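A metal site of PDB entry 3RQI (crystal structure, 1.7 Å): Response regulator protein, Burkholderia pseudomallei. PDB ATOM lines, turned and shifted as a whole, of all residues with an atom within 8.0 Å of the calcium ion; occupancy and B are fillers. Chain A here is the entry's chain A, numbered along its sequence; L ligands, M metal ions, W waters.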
ATOM      1  N   ILE A  13     -18.144   4.571  17.519  1.00  0.00           N
ATOM      2  CA  ILE A  13     -17.081   5.499  17.060  1.00  0.00           C
ATOM      3  C   ILE A  13     -15.813   5.189  17.865  1.00  0.00           C
ATOM      4  O   ILE A  13     -15.722   5.509  19.058  1.00  0.00           O
ATOM      5  CB  ILE A  13     -17.483   6.951  17.301  1.00  0.00           C
ATOM      6  CG1 ILE A  13     -18.793   7.268  16.546  1.00  0.00           C
ATOM      7  CG2 ILE A  13     -16.324   7.890  16.847  1.00  0.00           C
ATOM      8  CD1 ILE A  13     -19.488   8.530  17.077  1.00  0.00           C
ATOM      9  N   ASP A  14     -14.838   4.550  17.214  1.00  0.00           N
ATOM     10  CA  ASP A  14     -13.566   4.204  17.871  1.00  0.00           C
ATOM     11  C   ASP A  14     -12.534   3.981  16.768  1.00  0.00           C
ATOM     12  O   ASP A  14     -12.842   3.353  15.753  1.00  0.00           O
ATOM     13  CB  ASP A  14     -13.762   2.924  18.747  1.00  0.00           C
ATOM     14  CG  ASP A  14     -12.681   2.755  19.749  1.00  0.00           C
ATOM     15  OD1 ASP A  14     -11.494   2.664  19.342  1.00  0.00           O
ATOM     16  OD2 ASP A  14     -12.975   2.753  20.974  1.00  0.00           O
ATOM     17  N   ASP A  15     -11.347   4.535  16.931  1.00  0.00           N
ATOM     18  CA  ASP A  15     -10.309   4.362  15.878  1.00  0.00           C
ATOM     19  C   ASP A  15      -9.687   2.974  15.861  1.00  0.00           C
ATOM     20  O   ASP A  15      -8.978   2.614  14.889  1.00  0.00           O
ATOM     21  CB  ASP A  15      -9.184   5.399  16.093  1.00  0.00           C
ATOM     22  CG  ASP A  15      -8.431   5.158  17.369  1.00  0.00           C
ATOM     23  OD1 ASP A  15      -9.027   5.318  18.467  1.00  0.00           O
ATOM     24  OD2 ASP A  15      -7.247   4.825  17.304  1.00  0.00           O
ATOM     25  N   ASN A  16      -9.877   2.211  16.956  1.00  0.00           N
ATOM     26  CA  ASN A  16      -9.349   0.846  17.037  1.00  0.00           C
ATOM     27  C   ASN A  16     -10.371  -0.065  16.364  1.00  0.00           C
ATOM     28  O   ASN A  16     -11.389  -0.397  16.954  1.00  0.00           O
ATOM     29  CB  ASN A  16      -9.117   0.498  18.524  1.00  0.00           C
ATOM     30  CG  ASN A  16      -8.622  -0.936  18.757  1.00  0.00           C
ATOM     31  OD1 ASN A  16      -8.757  -1.818  17.907  1.00  0.00           O
ATOM     32  ND2 ASN A  16      -8.091  -1.161  19.954  1.00  0.00           N
ATOM     33  N   PHE A  19     -11.091  -3.604  18.153  1.00  0.00           N
ATOM     34  CA  PHE A  19     -12.016  -3.405  19.241  1.00  0.00           C
ATOM     35  C   PHE A  19     -13.422  -3.094  18.724  1.00  0.00           C
ATOM     36  O   PHE A  19     -14.390  -3.645  19.219  1.00  0.00           O
ATOM     37  CB  PHE A  19     -11.518  -2.279  20.158  1.00  0.00           C
ATOM     38  CG  PHE A  19     -12.497  -1.901  21.226  1.00  0.00           C
ATOM     39  CD1 PHE A  19     -12.506  -2.590  22.434  1.00  0.00           C
ATOM     40  CD2 PHE A  19     -13.432  -0.893  21.011  1.00  0.00           C
ATOM     41  CE1 PHE A  19     -13.403  -2.264  23.417  1.00  0.00           C
ATOM     42  CE2 PHE A  19     -14.363  -0.579  22.020  1.00  0.00           C
ATOM     43  CZ  PHE A  19     -14.335  -1.277  23.195  1.00  0.00           C
ATOM     44  N   HIS A  38     -14.282   5.332  12.378  1.00  0.00           N
ATOM     45  CA  HIS A  38     -12.937   5.181  12.968  1.00  0.00           C
ATOM     46  C   HIS A  38     -12.217   6.503  13.124  1.00  0.00           C
ATOM     47  O   HIS A  38     -11.084   6.542  13.615  1.00  0.00           O
ATOM     48  CB  HIS A  38     -12.077   4.180  12.156  1.00  0.00           C
ATOM     49  CG  HIS A  38     -12.777   2.870  11.947  1.00  0.00           C
ATOM     50  ND1 HIS A  38     -12.856   2.257  10.708  1.00  0.00           N
ATOM     51  CD2 HIS A  38     -13.466   2.095  12.810  1.00  0.00           C
ATOM     52  CE1 HIS A  38     -13.557   1.141  10.838  1.00  0.00           C
ATOM     53  NE2 HIS A  38     -13.954   1.030  12.089  1.00  0.00           N
ATOM     54  N   PHD A  58     -15.385   6.988  21.613  1.00  0.00           N
ATOM     55  CA  PHD A  58     -14.033   6.899  22.163  1.00  0.00           C
ATOM     56  C   PHD A  58     -13.478   8.295  22.317  1.00  0.00           C
ATOM     57  O   PHD A  58     -13.764   9.160  21.485  1.00  0.00           O
ATOM     58  CB  PHD A  58     -13.252   6.108  21.080  1.00  0.00           C
ATOM     59  CG  PHD A  58     -11.824   5.818  21.479  1.00  0.00           C
ATOM     60  OD1 PHD A  58     -11.632   5.502  22.861  1.00  0.00           O
ATOM     61  OD2 PHD A  58     -10.895   5.791  20.640  1.00  0.00           O
ATOM     62  P   PHD A  58     -10.285   5.692  23.766  1.00  0.00           P
ATOM     63  OP1 PHD A  58     -10.359   4.386  24.534  1.00  0.00           O
ATOM     64  OP2 PHD A  58      -9.116   5.872  22.859  1.00  0.00           O
ATOM     65  OP3 PHD A  58     -10.664   6.918  24.544  1.00  0.00           O
ATOM     66  N   LEU A  59     -12.709   8.567  23.363  1.00  0.00           N
ATOM     67  CA  LEU A  59     -12.159   9.917  23.535  1.00  0.00           C
ATOM     68  C   LEU A  59     -10.897  10.145  22.725  1.00  0.00           C
ATOM     69  O   LEU A  59     -10.757  11.184  22.062  1.00  0.00           O
ATOM     70  CB  LEU A  59     -11.857  10.211  25.025  1.00  0.00           C
ATOM     71  CG  LEU A  59     -13.119  10.236  25.885  1.00  0.00           C
ATOM     72  CD1 LEU A  59     -12.753  10.509  27.343  1.00  0.00           C
ATOM     73  CD2 LEU A  59     -14.158  11.247  25.359  1.00  0.00           C
ATOM     74  N   HIS A  60      -9.947   9.226  22.821  1.00  0.00           N
ATOM     75  CA  HIS A  60      -8.706   9.376  22.112  1.00  0.00           C
ATOM     76  C   HIS A  60      -8.869   8.793  20.738  1.00  0.00           C
ATOM     77  O   HIS A  60      -8.410   7.680  20.447  1.00  0.00           O
ATOM     78  CB  HIS A  60      -7.564   8.718  22.874  1.00  0.00           C
ATOM     79  CG  HIS A  60      -6.233   9.151  22.390  1.00  0.00           C
ATOM     80  ND1 HIS A  60      -5.543   8.461  21.412  1.00  0.00           N
ATOM     81  CD2 HIS A  60      -5.474  10.221  22.716  1.00  0.00           C
ATOM     82  CE1 HIS A  60      -4.399   9.087  21.167  1.00  0.00           C
ATOM     83  NE2 HIS A  60      -4.334  10.153  21.944  1.00  0.00           N
ATOM     84  N   LEU A  61      -9.520   9.568  19.873  1.00  0.00           N
ATOM     85  CA  LEU A  61      -9.923   9.053  18.572  1.00  0.00           C
ATOM     86  C   LEU A  61      -8.825   9.210  17.516  1.00  0.00           C
ATOM     87  O   LEU A  61      -9.021   9.914  16.548  1.00  0.00           O
ATOM     88  CB  LEU A  61     -11.252   9.687  18.129  1.00  0.00           C
ATOM     89  CG  LEU A  61     -12.064   9.152  16.958  1.00  0.00           C
ATOM     90  CD1 LEU A  61     -12.579   7.721  17.306  1.00  0.00           C
ATOM     91  CD2 LEU A  61     -13.255  10.068  16.740  1.00  0.00           C
ATOM     92  N   GLY A  62      -7.741   8.470  17.663  1.00  0.00           N
ATOM     93  CA  GLY A  62      -6.611   8.602  16.734  1.00  0.00           C
ATOM     94  C   GLY A  62      -6.090  10.017  16.802  1.00  0.00           C
ATOM     95  O   GLY A  62      -5.740  10.478  17.865  1.00  0.00           O
ATOM     96  N   ASN A  63      -6.077  10.724  15.663  1.00  0.00           N
ATOM     97  CA  ASN A  63      -5.653  12.146  15.614  1.00  0.00           C
ATOM     98  C   ASN A  63      -6.773  13.118  16.073  1.00  0.00           C
ATOM     99  O   ASN A  63      -6.565  14.348  16.197  1.00  0.00           O
ATOM    100  CB  ASN A  63      -5.251  12.468  14.170  1.00  0.00           C
ATOM    101  CG  ASN A  63      -4.539  13.812  14.007  1.00  0.00           C
ATOM    102  OD1 ASN A  63      -3.488  14.064  14.630  1.00  0.00           O
ATOM    103  ND2 ASN A  63      -5.076  14.653  13.108  1.00  0.00           N
ATOM    104  N   ASP A  64      -7.968  12.574  16.319  1.00  0.00           N
ATOM    105  CA  ASP A  64      -9.170  13.399  16.601  1.00  0.00           C
ATOM    106  C   ASP A  64      -9.607  13.385  18.074  1.00  0.00           C
ATOM    107  O   ASP A  64      -9.257  12.491  18.830  1.00  0.00           O
ATOM    108  CB  ASP A  64     -10.311  12.934  15.683  1.00  0.00           C
ATOM    109  CG  ASP A  64      -9.942  13.024  14.223  1.00  0.00           C
ATOM    110  OD1 ASP A  64      -9.174  13.959  13.875  1.00  0.00           O
ATOM    111  OD2 ASP A  64     -10.381  12.168  13.418  1.00  0.00           O
ATOM    112  N   LEU A  85     -17.149   5.783  25.890  1.00  0.00           N
ATOM    113  CA  LEU A  85     -16.555   4.476  26.267  1.00  0.00           C
ATOM    114  C   LEU A  85     -15.039   4.577  26.021  1.00  0.00           C
ATOM    115  O   LEU A  85     -14.603   4.695  24.860  1.00  0.00           O
ATOM    116  CB  LEU A  85     -17.194   3.340  25.436  1.00  0.00           C
ATOM    117  CG  LEU A  85     -16.595   1.932  25.658  1.00  0.00           C
ATOM    118  CD1 LEU A  85     -16.747   1.519  27.121  1.00  0.00           C
ATOM    119  CD2 LEU A  85     -17.288   0.943  24.744  1.00  0.00           C
ATOM    120  N   THR A  86     -14.238   4.626  27.107  1.00  0.00           N
ATOM    121  CA  THR A  86     -12.830   5.087  26.966  1.00  0.00           C
ATOM    122  C   THR A  86     -11.798   4.329  27.789  1.00  0.00           C
ATOM    123  O   THR A  86     -12.059   3.990  28.952  1.00  0.00           O
ATOM    124  CB  THR A  86     -12.681   6.614  27.255  1.00  0.00           C
ATOM    125  OG1 THR A  86     -11.337   7.043  27.105  1.00  0.00           O
ATOM    126  CG2 THR A  86     -13.159   6.979  28.625  1.00  0.00           C
ATOM    127  N   GLY A  87     -10.640   4.101  27.179  1.00  0.00           N
ATOM    128  CA  GLY A  87      -9.475   3.541  27.886  1.00  0.00           C
ATOM    129  C   GLY A  87      -8.640   4.620  28.579  1.00  0.00           C
ATOM    130  O   GLY A  87      -7.616   4.324  29.202  1.00  0.00           O
ATOM    131  N   TYR A  88      -9.105   5.882  28.481  1.00  0.00           N
ATOM    132  CA  TYR A  88      -8.452   6.995  29.120  1.00  0.00           C
ATOM    133  C   TYR A  88      -9.370   7.715  30.121  1.00  0.00           C
ATOM    134  O   TYR A  88      -9.597   8.919  30.023  1.00  0.00           O
ATOM    135  CB  TYR A  88      -7.910   7.942  28.071  1.00  0.00           C
ATOM    136  CG  TYR A  88      -6.885   7.271  27.196  1.00  0.00           C
ATOM    137  CD1 TYR A  88      -5.584   7.032  27.649  1.00  0.00           C
ATOM    138  CD2 TYR A  88      -7.245   6.821  25.932  1.00  0.00           C
ATOM    139  CE1 TYR A  88      -4.651   6.384  26.817  1.00  0.00           C
ATOM    140  CE2 TYR A  88      -6.348   6.191  25.122  1.00  0.00           C
ATOM    141  CZ  TYR A  88      -5.053   5.964  25.557  1.00  0.00           C
ATOM    142  OH  TYR A  88      -4.171   5.338  24.694  1.00  0.00           O
ATOM    143  N   LYS A 108     -13.306   1.547  29.686  1.00  0.00           N
ATOM    144  CA  LYS A 108     -12.868   0.248  29.169  1.00  0.00           C
ATOM    145  C   LYS A 108     -11.968  -0.445  30.240  1.00  0.00           C
ATOM    146  O   LYS A 108     -11.256   0.238  31.006  1.00  0.00           O
ATOM    147  CB  LYS A 108     -12.072   0.383  27.864  1.00  0.00           C
ATOM    148  CG  LYS A 108     -12.808   0.991  26.686  1.00  0.00           C
ATOM    149  CD  LYS A 108     -11.850   1.115  25.496  1.00  0.00           C
ATOM    150  CE  LYS A 108     -12.560   1.732  24.273  1.00  0.00           C
ATOM    151  NZ  LYS A 108     -11.496   2.157  23.314  1.00  0.00           N
HETATM  152  C1  LIG L   1      -5.118   5.777  19.461  1.00  0.00           C
HETATM  153  O1  LIG L   1      -6.243   6.108  19.928  1.00  0.00           O
HETATM  154  O2  LIG L   1      -4.385   6.687  19.028  1.00  0.00           O
HETATM  155  C2  LIG L   1      -4.686   4.315  19.432  1.00  0.00           C
HETATM  156  C3  LIG L   1      -5.661   3.465  20.267  1.00  0.00           C
HETATM  157  O3  LIG L   1      -6.995   3.633  19.700  1.00  0.00           O
HETATM  158  C4  LIG L   1      -5.314   1.975  20.193  1.00  0.00           C
HETATM  159  C5  LIG L   1      -6.034   1.084  21.180  1.00  0.00           C
HETATM  160  O4  LIG L   1      -5.370   0.115  21.643  1.00  0.00           O
HETATM  161  O5  LIG L   1      -7.247   1.258  21.552  1.00  0.00           O
HETATM  162  C6  LIG L   1      -5.613   3.996  21.693  1.00  0.00           C
HETATM  163  O6  LIG L   1      -4.538   4.092  22.355  1.00  0.00           O
HETATM  164  O7  LIG L   1      -6.680   4.359  22.217  1.00  0.00           O
HETATM  165 CA    CA M   1      -8.520   5.275  20.750  1.00  0.00          CA
HETATM  166  O   HOH W   1      -9.507   3.132  21.083  1.00  0.00           O
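Within 4 Å of the calcium ion: Asp 15, PHD 58 and His 60.
Water W1 bridges the side-chain carboxylate of Asp 14 (2.7 Å) and the side-chain amino group of Lys 108 (3.1 Å).
OP1 of PHD 58 lies within salt-bridge range of the side-chain amino group of Lys 108, 2.8 Å away. OP1 of PHD 58 sits at hydrogen-bond distance from N of Gly 87 (2.7 Å). OP3 of PHD 58 sits at hydrogen-bond distance from OG1 of Thr 86. N of PHD 58 lies within hydrogen-bond range of O of Ile 13 (3.0 Å). The side-chain carboxylate of Asp 15 sits close to the backbone NH of Gly 62, at 3.5 Å.
The calcium ion is bound by OP2 of PHD 58, the side-chain carboxylate of Asp 15, water W1, the backbone carbonyl oxygen of His 60, OD2 of PHD 58, an oxygen (O3) of the ligand, an oxygen (O7) of the ligand and an oxygen (O1) of the ligand. The calcium ion has eight donor atoms within binding distance.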
